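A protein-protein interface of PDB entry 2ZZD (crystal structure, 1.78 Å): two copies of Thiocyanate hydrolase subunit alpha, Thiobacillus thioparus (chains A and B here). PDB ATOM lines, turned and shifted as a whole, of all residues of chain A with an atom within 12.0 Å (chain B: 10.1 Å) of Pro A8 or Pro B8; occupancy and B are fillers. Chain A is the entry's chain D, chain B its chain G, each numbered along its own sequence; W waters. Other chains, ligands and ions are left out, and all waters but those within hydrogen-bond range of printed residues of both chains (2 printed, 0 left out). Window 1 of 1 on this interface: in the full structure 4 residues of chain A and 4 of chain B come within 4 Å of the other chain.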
ATOM      1  N   LYS A   7      21.458 -38.577 -18.207  1.00  0.00           N
ATOM      2  CA  LYS A   7      22.284 -37.478 -17.628  1.00  0.00           C
ATOM      3  C   LYS A   7      21.445 -36.225 -17.453  1.00  0.00           C
ATOM      4  O   LYS A   7      20.398 -36.075 -18.083  1.00  0.00           O
ATOM      5  CB  LYS A   7      23.475 -37.160 -18.538  1.00  0.00           C
ATOM      6  CG  LYS A   7      24.459 -38.302 -18.684  1.00  0.00           C
ATOM      7  CD  LYS A   7      23.854 -39.438 -19.480  1.00  0.00           C
ATOM      8  CE  LYS A   7      24.225 -40.777 -18.884  1.00  0.00           C
ATOM      9  NZ  LYS A   7      23.597 -41.878 -19.655  1.00  0.00           N
ATOM     10  N   PRO A   8      21.883 -35.309 -16.580  1.00  0.00           N
ATOM     11  CA  PRO A   8      21.082 -34.099 -16.412  1.00  0.00           C
ATOM     12  C   PRO A   8      21.090 -33.222 -17.664  1.00  0.00           C
ATOM     13  O   PRO A   8      22.044 -33.241 -18.448  1.00  0.00           O
ATOM     14  CB  PRO A   8      21.731 -33.421 -15.205  1.00  0.00           C
ATOM     15  CG  PRO A   8      23.156 -33.871 -15.289  1.00  0.00           C
ATOM     16  CD  PRO A   8      23.007 -35.334 -15.627  1.00  0.00           C
ATOM     17  N   VAL A   9      20.003 -32.482 -17.854  1.00  0.00           N
ATOM     18  CA  VAL A   9      19.867 -31.574 -18.982  1.00  0.00           C
ATOM     19  C   VAL A   9      19.891 -30.163 -18.423  1.00  0.00           C
ATOM     20  O   VAL A   9      19.227 -29.866 -17.429  1.00  0.00           O
ATOM     21  CB  VAL A   9      18.533 -31.769 -19.734  1.00  0.00           C
ATOM     22  CG1 VAL A   9      18.341 -30.643 -20.741  1.00  0.00           C
ATOM     23  CG2 VAL A   9      18.524 -33.112 -20.445  1.00  0.00           C
ATOM     24  N   TRP A  10      20.674 -29.304 -19.063  1.00  0.00           N
ATOM     25  CA  TRP A  10      20.790 -27.921 -18.643  1.00  0.00           C
ATOM     26  C   TRP A  10      19.973 -27.026 -19.545  1.00  0.00           C
ATOM     27  O   TRP A  10      20.107 -27.078 -20.767  1.00  0.00           O
ATOM     28  CB  TRP A  10      22.249 -27.491 -18.680  1.00  0.00           C
ATOM     29  CG  TRP A  10      23.062 -28.324 -17.783  1.00  0.00           C
ATOM     30  CD1 TRP A  10      23.722 -29.480 -18.097  1.00  0.00           C
ATOM     31  CD2 TRP A  10      23.188 -28.158 -16.376  1.00  0.00           C
ATOM     32  NE1 TRP A  10      24.244 -30.048 -16.960  1.00  0.00           N
ATOM     33  CE2 TRP A  10      23.930 -29.254 -15.889  1.00  0.00           C
ATOM     34  CE3 TRP A  10      22.741 -27.186 -15.474  1.00  0.00           C
ATOM     35  CZ2 TRP A  10      24.230 -29.406 -14.537  1.00  0.00           C
ATOM     36  CZ3 TRP A  10      23.038 -27.338 -14.138  1.00  0.00           C
ATOM     37  CH2 TRP A  10      23.776 -28.438 -13.681  1.00  0.00           C
ATOM     38  N   ASP A  11      19.125 -26.204 -18.941  1.00  0.00           N
ATOM     39  CA  ASP A  11      18.300 -25.288 -19.713  1.00  0.00           C
ATOM     40  C   ASP A  11      19.130 -24.071 -20.107  1.00  0.00           C
ATOM     41  O   ASP A  11      19.359 -23.176 -19.293  1.00  0.00           O
ATOM     42  CB  ASP A  11      17.095 -24.835 -18.897  1.00  0.00           C
ATOM     43  CG  ASP A  11      16.137 -23.995 -19.712  1.00  0.00           C
ATOM     44  OD1 ASP A  11      16.543 -23.509 -20.789  1.00  0.00           O
ATOM     45  OD2 ASP A  11      14.980 -23.809 -19.280  1.00  0.00           O
ATOM     46  N   ARG A  12      19.564 -24.034 -21.361  1.00  0.00           N
ATOM     47  CA  ARG A  12      20.384 -22.932 -21.852  1.00  0.00           C
ATOM     48  C   ARG A  12      19.602 -21.759 -22.431  1.00  0.00           C
ATOM     49  O   ARG A  12      20.201 -20.805 -22.929  1.00  0.00           O
ATOM     50  CB  ARG A  12      21.363 -23.444 -22.908  1.00  0.00           C
ATOM     51  CG  ARG A  12      22.489 -24.297 -22.349  1.00  0.00           C
ATOM     52  CD  ARG A  12      23.455 -24.708 -23.446  1.00  0.00           C
ATOM     53  NE  ARG A  12      23.072 -25.965 -24.082  1.00  0.00           N
ATOM     54  CZ  ARG A  12      23.215 -26.217 -25.378  1.00  0.00           C
ATOM     55  NH1 ARG A  12      23.723 -25.291 -26.180  1.00  0.00           N
ATOM     56  NH2 ARG A  12      22.874 -27.400 -25.873  1.00  0.00           N
ATOM     57  N   THR A  13      18.275 -21.812 -22.366  1.00  0.00           N
ATOM     58  CA  THR A  13      17.462 -20.726 -22.917  1.00  0.00           C
ATOM     59  C   THR A  13      16.736 -19.892 -21.862  1.00  0.00           C
ATOM     60  O   THR A  13      16.260 -18.793 -22.157  1.00  0.00           O
ATOM     61  CB  THR A  13      16.396 -21.272 -23.892  1.00  0.00           C
ATOM     62  OG1 THR A  13      15.453 -22.072 -23.170  1.00  0.00           O
ATOM     63  CG2 THR A  13      17.047 -22.118 -24.976  1.00  0.00           C
ATOM     64  N   HIS A  14      16.657 -20.402 -20.636  1.00  0.00           N
ATOM     65  CA  HIS A  14      15.952 -19.702 -19.566  1.00  0.00           C
ATOM     66  C   HIS A  14      16.328 -18.240 -19.327  1.00  0.00           C
ATOM     67  O   HIS A  14      15.463 -17.362 -19.348  1.00  0.00           O
ATOM     68  CB  HIS A  14      16.100 -20.447 -18.240  1.00  0.00           C
ATOM     69  CG  HIS A  14      15.448 -19.747 -17.089  1.00  0.00           C
ATOM     70  ND1 HIS A  14      14.079 -19.660 -16.950  1.00  0.00           N
ATOM     71  CD2 HIS A  14      15.975 -19.050 -16.055  1.00  0.00           C
ATOM     72  CE1 HIS A  14      13.791 -18.939 -15.881  1.00  0.00           C
ATOM     73  NE2 HIS A  14      14.925 -18.557 -15.320  1.00  0.00           N
ATOM     74  N   ASP A  79      23.032 -17.701  -4.147  1.00  0.00           N
ATOM     75  CA  ASP A  79      22.128 -18.655  -4.786  1.00  0.00           C
ATOM     76  C   ASP A  79      22.345 -18.665  -6.302  1.00  0.00           C
ATOM     77  O   ASP A  79      22.458 -19.722  -6.924  1.00  0.00           O
ATOM     78  CB  ASP A  79      20.663 -18.313  -4.473  1.00  0.00           C
ATOM     79  CG  ASP A  79      20.279 -18.636  -3.040  1.00  0.00           C
ATOM     80  OD1 ASP A  79      20.756 -19.664  -2.508  1.00  0.00           O
ATOM     81  OD2 ASP A  79      19.487 -17.872  -2.445  1.00  0.00           O
ATOM     82  N   GLU A  80      22.430 -17.477  -6.889  1.00  0.00           N
ATOM     83  CA  GLU A  80      22.620 -17.354  -8.328  1.00  0.00           C
ATOM     84  C   GLU A  80      23.869 -18.101  -8.808  1.00  0.00           C
ATOM     85  O   GLU A  80      23.852 -18.740  -9.863  1.00  0.00           O
ATOM     86  CB  GLU A  80      22.704 -15.870  -8.704  1.00  0.00           C
ATOM     87  CG  GLU A  80      22.431 -15.570 -10.171  1.00  0.00           C
ATOM     88  CD  GLU A  80      22.349 -14.082 -10.437  1.00  0.00           C
ATOM     89  OE1 GLU A  80      23.323 -13.374 -10.108  1.00  0.00           O
ATOM     90  OE2 GLU A  80      21.314 -13.616 -10.965  1.00  0.00           O
ATOM     91  N   ALA A  81      24.943 -18.037  -8.024  1.00  0.00           N
ATOM     92  CA  ALA A  81      26.195 -18.694  -8.390  1.00  0.00           C
ATOM     93  C   ALA A  81      26.133 -20.222  -8.400  1.00  0.00           C
ATOM     94  O   ALA A  81      27.067 -20.875  -8.862  1.00  0.00           O
ATOM     95  CB  ALA A  81      27.324 -18.227  -7.470  1.00  0.00           C
ATOM     96  N   PHE A  82      25.048 -20.791  -7.879  1.00  0.00           N
ATOM     97  CA  PHE A  82      24.889 -22.239  -7.871  1.00  0.00           C
ATOM     98  C   PHE A  82      23.667 -22.653  -8.686  1.00  0.00           C
ATOM     99  O   PHE A  82      23.180 -23.779  -8.582  1.00  0.00           O
ATOM    100  CB  PHE A  82      24.818 -22.756  -6.431  1.00  0.00           C
ATOM    101  CG  PHE A  82      26.159 -22.772  -5.748  1.00  0.00           C
ATOM    102  CD1 PHE A  82      27.062 -23.805  -5.991  1.00  0.00           C
ATOM    103  CD2 PHE A  82      26.556 -21.713  -4.941  1.00  0.00           C
ATOM    104  CE1 PHE A  82      28.344 -23.779  -5.446  1.00  0.00           C
ATOM    105  CE2 PHE A  82      27.839 -21.679  -4.391  1.00  0.00           C
ATOM    106  CZ  PHE A  82      28.734 -22.714  -4.647  1.00  0.00           C
ATOM    107  N   GLY A  83      23.194 -21.723  -9.512  1.00  0.00           N
ATOM    108  CA  GLY A  83      22.056 -21.983 -10.381  1.00  0.00           C
ATOM    109  C   GLY A  83      20.686 -21.941  -9.735  1.00  0.00           C
ATOM    110  O   GLY A  83      19.714 -22.437 -10.310  1.00  0.00           O
ATOM    111  N   ASN A  84      20.602 -21.336  -8.556  1.00  0.00           N
ATOM    112  CA  ASN A  84      19.344 -21.245  -7.816  1.00  0.00           C
ATOM    113  C   ASN A  84      18.814 -19.814  -7.873  1.00  0.00           C
ATOM    114  O   ASN A  84      19.320 -18.934  -7.178  1.00  0.00           O
ATOM    115  CB  ASN A  84      19.588 -21.663  -6.360  1.00  0.00           C
ATOM    116  CG  ASN A  84      20.247 -23.031  -6.254  1.00  0.00           C
ATOM    117  OD1 ASN A  84      21.219 -23.221  -5.514  1.00  0.00           O
ATOM    118  ND2 ASN A  84      19.716 -23.995  -6.993  1.00  0.00           N
ATOM    119  N   GLU A  85      17.794 -19.581  -8.699  1.00  0.00           N
ATOM    120  CA  GLU A  85      17.232 -18.237  -8.849  1.00  0.00           C
ATOM    121  C   GLU A  85      15.764 -18.116  -8.419  1.00  0.00           C
ATOM    122  O   GLU A  85      15.121 -17.095  -8.690  1.00  0.00           O
ATOM    123  CB  GLU A  85      17.376 -17.773 -10.307  1.00  0.00           C
ATOM    124  CG  GLU A  85      18.818 -17.784 -10.818  1.00  0.00           C
ATOM    125  CD  GLU A  85      18.951 -17.282 -12.248  1.00  0.00           C
ATOM    126  OE1 GLU A  85      17.920 -16.950 -12.876  1.00  0.00           O
ATOM    127  OE2 GLU A  85      20.097 -17.229 -12.747  1.00  0.00           O
ATOM    128  N   GLU A  86      15.245 -19.140  -7.739  1.00  0.00           N
ATOM    129  CA  GLU A  86      13.851 -19.149  -7.287  1.00  0.00           C
ATOM    130  C   GLU A  86      13.505 -18.041  -6.297  1.00  0.00           C
ATOM    131  O   GLU A  86      12.362 -17.579  -6.249  1.00  0.00           O
ATOM    132  CB  GLU A  86      13.506 -20.494  -6.641  1.00  0.00           C
ATOM    133  CG  GLU A  86      13.606 -21.705  -7.562  1.00  0.00           C
ATOM    134  CD  GLU A  86      15.035 -22.154  -7.789  1.00  0.00           C
ATOM    135  OE1 GLU A  86      15.915 -21.777  -6.983  1.00  0.00           O
ATOM    136  OE2 GLU A  86      15.275 -22.899  -8.763  1.00  0.00           O
ATOM    137  N   LYS B   7      16.810 -26.884 -12.659  1.00  0.00           N
ATOM    138  CA  LYS B   7      16.187 -27.813 -13.647  1.00  0.00           C
ATOM    139  C   LYS B   7      16.798 -29.204 -13.722  1.00  0.00           C
ATOM    140  O   LYS B   7      16.079 -30.198 -13.787  1.00  0.00           O
ATOM    141  CB  LYS B   7      16.240 -27.214 -15.056  1.00  0.00           C
ATOM    142  CG  LYS B   7      15.243 -26.120 -15.304  1.00  0.00           C
ATOM    143  CD  LYS B   7      13.829 -26.659 -15.252  1.00  0.00           C
ATOM    144  CE  LYS B   7      12.822 -25.537 -15.383  1.00  0.00           C
ATOM    145  NZ  LYS B   7      12.814 -24.685 -14.161  1.00  0.00           N
ATOM    146  N   PRO B   8      18.134 -29.297 -13.682  1.00  0.00           N
ATOM    147  CA  PRO B   8      18.721 -30.633 -13.778  1.00  0.00           C
ATOM    148  C   PRO B   8      18.200 -31.634 -12.766  1.00  0.00           C
ATOM    149  O   PRO B   8      17.997 -31.313 -11.593  1.00  0.00           O
ATOM    150  CB  PRO B   8      20.222 -30.390 -13.606  1.00  0.00           C
ATOM    151  CG  PRO B   8      20.375 -28.892 -13.432  1.00  0.00           C
ATOM    152  CD  PRO B   8      19.055 -28.384 -12.988  1.00  0.00           C
ATOM    153  N   VAL B   9      17.970 -32.848 -13.250  1.00  0.00           N
ATOM    154  CA  VAL B   9      17.513 -33.948 -12.419  1.00  0.00           C
ATOM    155  C   VAL B   9      18.613 -34.996 -12.445  1.00  0.00           C
ATOM    156  O   VAL B   9      19.082 -35.398 -13.514  1.00  0.00           O
ATOM    157  CB  VAL B   9      16.223 -34.590 -12.960  1.00  0.00           C
ATOM    158  CG1 VAL B   9      15.907 -35.848 -12.168  1.00  0.00           C
ATOM    159  CG2 VAL B   9      15.072 -33.609 -12.861  1.00  0.00           C
ATOM    160  N   TRP B  10      19.037 -35.423 -11.262  1.00  0.00           N
ATOM    161  CA  TRP B  10      20.077 -36.430 -11.162  1.00  0.00           C
ATOM    162  C   TRP B  10      19.460 -37.797 -10.925  1.00  0.00           C
ATOM    163  O   TRP B  10      18.588 -37.957 -10.070  1.00  0.00           O
ATOM    164  CB  TRP B  10      21.043 -36.081 -10.031  1.00  0.00           C
ATOM    165  CG  TRP B  10      21.673 -34.749 -10.245  1.00  0.00           C
ATOM    166  CD1 TRP B  10      21.216 -33.543  -9.795  1.00  0.00           C
ATOM    167  CD2 TRP B  10      22.809 -34.466 -11.066  1.00  0.00           C
ATOM    168  NE1 TRP B  10      21.992 -32.525 -10.291  1.00  0.00           N
ATOM    169  CE2 TRP B  10      22.978 -33.064 -11.076  1.00  0.00           C
ATOM    170  CE3 TRP B  10      23.698 -35.261 -11.803  1.00  0.00           C
ATOM    171  CZ2 TRP B  10      24.000 -32.439 -11.789  1.00  0.00           C
ATOM    172  CZ3 TRP B  10      24.715 -34.638 -12.512  1.00  0.00           C
ATOM    173  CH2 TRP B  10      24.856 -33.239 -12.500  1.00  0.00           C
ATOM    174  N   ASP B  11      19.908 -38.776 -11.703  1.00  0.00           N
ATOM    175  CA  ASP B  11      19.413 -40.140 -11.580  1.00  0.00           C
ATOM    176  C   ASP B  11      20.132 -40.826 -10.423  1.00  0.00           C
ATOM    177  O   ASP B  11      21.282 -41.243 -10.564  1.00  0.00           O
ATOM    178  CB  ASP B  11      19.680 -40.917 -12.869  1.00  0.00           C
ATOM    179  CG  ASP B  11      19.117 -42.325 -12.826  1.00  0.00           C
ATOM    180  OD1 ASP B  11      18.891 -42.842 -11.713  1.00  0.00           O
ATOM    181  OD2 ASP B  11      18.907 -42.920 -13.904  1.00  0.00           O
ATOM    182  N   ARG B  12      19.457 -40.965  -9.288  1.00  0.00           N
ATOM    183  CA  ARG B  12      20.074 -41.592  -8.123  1.00  0.00           C
ATOM    184  C   ARG B  12      19.924 -43.111  -8.025  1.00  0.00           C
ATOM    185  O   ARG B  12      20.381 -43.715  -7.052  1.00  0.00           O
ATOM    186  CB  ARG B  12      19.542 -40.943  -6.841  1.00  0.00           C
ATOM    187  CG  ARG B  12      20.041 -39.514  -6.628  1.00  0.00           C
ATOM    188  CD  ARG B  12      19.550 -38.951  -5.309  1.00  0.00           C
ATOM    189  NE  ARG B  12      18.306 -38.202  -5.448  1.00  0.00           N
ATOM    190  CZ  ARG B  12      17.358 -38.164  -4.519  1.00  0.00           C
ATOM    191  NH1 ARG B  12      17.510 -38.845  -3.391  1.00  0.00           N
ATOM    192  NH2 ARG B  12      16.267 -37.434  -4.709  1.00  0.00           N
ATOM    193  N   HIS B  14      20.491 -45.298 -11.002  1.00  0.00           N
ATOM    194  CA  HIS B  14      21.250 -45.973 -12.049  1.00  0.00           C
ATOM    195  C   HIS B  14      22.336 -46.952 -11.599  1.00  0.00           C
ATOM    196  O   HIS B  14      22.333 -48.116 -12.003  1.00  0.00           O
ATOM    197  CB  HIS B  14      21.876 -44.954 -13.003  1.00  0.00           C
ATOM    198  CG  HIS B  14      22.660 -45.585 -14.112  1.00  0.00           C
ATOM    199  ND1 HIS B  14      24.025 -45.764 -14.056  1.00  0.00           N
ATOM    200  CD2 HIS B  14      22.257 -46.142 -15.280  1.00  0.00           C
ATOM    201  CE1 HIS B  14      24.429 -46.404 -15.138  1.00  0.00           C
ATOM    202  NE2 HIS B  14      23.375 -46.646 -15.897  1.00  0.00           N
ATOM    203  N   PHE B  82      33.467 -37.707 -13.403  1.00  0.00           N
ATOM    204  CA  PHE B  82      32.674 -36.581 -13.878  1.00  0.00           C
ATOM    205  C   PHE B  82      31.292 -37.048 -14.318  1.00  0.00           C
ATOM    206  O   PHE B  82      30.571 -36.341 -15.027  1.00  0.00           O
ATOM    207  CB  PHE B  82      33.418 -35.858 -15.002  1.00  0.00           C
ATOM    208  CG  PHE B  82      34.523 -34.967 -14.501  1.00  0.00           C
ATOM    209  CD1 PHE B  82      34.236 -33.694 -14.017  1.00  0.00           C
ATOM    210  CD2 PHE B  82      35.837 -35.430 -14.437  1.00  0.00           C
ATOM    211  CE1 PHE B  82      35.238 -32.892 -13.469  1.00  0.00           C
ATOM    212  CE2 PHE B  82      36.846 -34.635 -13.889  1.00  0.00           C
ATOM    213  CZ  PHE B  82      36.544 -33.365 -13.404  1.00  0.00           C
ATOM    214  N   GLY B  83      30.934 -38.251 -13.871  1.00  0.00           N
ATOM    215  CA  GLY B  83      29.631 -38.819 -14.172  1.00  0.00           C
ATOM    216  C   GLY B  83      29.438 -39.365 -15.572  1.00  0.00           C
ATOM    217  O   GLY B  83      28.305 -39.541 -16.018  1.00  0.00           O
ATOM    218  N   ASN B  84      30.536 -39.647 -16.263  1.00  0.00           N
ATOM    219  CA  ASN B  84      30.470 -40.166 -17.627  1.00  0.00           C
ATOM    220  C   ASN B  84      30.898 -41.631 -17.642  1.00  0.00           C
ATOM    221  O   ASN B  84      32.090 -41.928 -17.609  1.00  0.00           O
ATOM    222  CB  ASN B  84      31.392 -39.340 -18.529  1.00  0.00           C
ATOM    223  CG  ASN B  84      31.089 -37.851 -18.462  1.00  0.00           C
ATOM    224  OD1 ASN B  84      31.993 -37.024 -18.301  1.00  0.00           O
ATOM    225  ND2 ASN B  84      29.816 -37.501 -18.591  1.00  0.00           N
ATOM    226  N   GLU B  86      29.630 -43.958 -20.066  1.00  0.00           N
ATOM    227  CA  GLU B  86      29.276 -44.549 -21.362  1.00  0.00           C
ATOM    228  C   GLU B  86      30.366 -45.431 -21.963  1.00  0.00           C
ATOM    229  O   GLU B  86      30.071 -46.410 -22.661  1.00  0.00           O
ATOM    230  CB  GLU B  86      28.937 -43.456 -22.379  1.00  0.00           C
ATOM    231  CG  GLU B  86      27.708 -42.616 -22.054  1.00  0.00           C
ATOM    232  CD  GLU B  86      27.965 -41.576 -20.982  1.00  0.00           C
ATOM    233  OE1 GLU B  86      29.147 -41.249 -20.741  1.00  0.00           O
ATOM    234  OE2 GLU B  86      26.986 -41.074 -20.390  1.00  0.00           O
HETATM  235  O   HOH W   1      17.114 -24.854 -10.245  1.00  0.00           O
HETATM  236  O   HOH W   2      17.804 -33.089 -16.173  1.00  0.00           O
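The side-chain amino group (NZ) of Lys A7 is in salt-bridge range of the side-chain carboxylate (OE2) of Glu B86, at 3.6 Å.
Hydrophobic or aromatic side chains of chain A that line the printed part of chain B: Pro A8 and Trp A10.
Lys A7 touches Glu B86, but with the chains exchanged Glu A86 does not touch Lys B7 (5.8 Å).
Pro A8 touches its own counterpart, Pro B8.
Pro A8 touches Val B9, and with the chains exchanged Val A9 touches Pro B8.
Pro A8 touches Trp B10, and with the chains exchanged Trp A10 touches Pro B8.
11 positions are printed for both chains.
Of the 6 pairs that touch across the chains among the printed residues, 5 have their exchanged pair printed and touching as well.
Of the printed residues of chain B, Pro A8 touches Pro B8 (3.7 Å), Val B9 (3.7 Å) and Trp B10 (3.3 Å).
Val A9 touches just one residue of chain B: Pro B8 (3.8 Å).
Of chain A, only Pro A8 (3.3 Å) comes within 4 Å of Trp B10.
Printed residues of chain A within 4 Å of Glu B86: Lys A7.
Of the printed residues of chain B, Trp A10 touches Pro B8.
Of the printed residues of chain B, Lys A7 touches Glu B86 (3.2 Å).
The nearest residue of chain B that does not touch Pro A8 is Asp B11 (6.1 Å).
The nearest residue of chain A that does not touch Pro B8 is Asp A11 (6.2 Å).
Water W2 lies within hydrogen-bond range of N of Val A9 and N of Val B9.
Water W1 bridges the side-chain carboxylate of Glu A86 and the backbone NH of Lys B7.
Among the printed residues, pairs that only touch across the chains: Pro A8 with Pro B8 (3.7 Å), Pro A8 with Val B9 (3.7 Å), Pro A8 with Trp B10 (3.3 Å), Val A9 with Pro B8 (3.8 Å) and Trp A10 with Pro B8 (3.2 Å).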
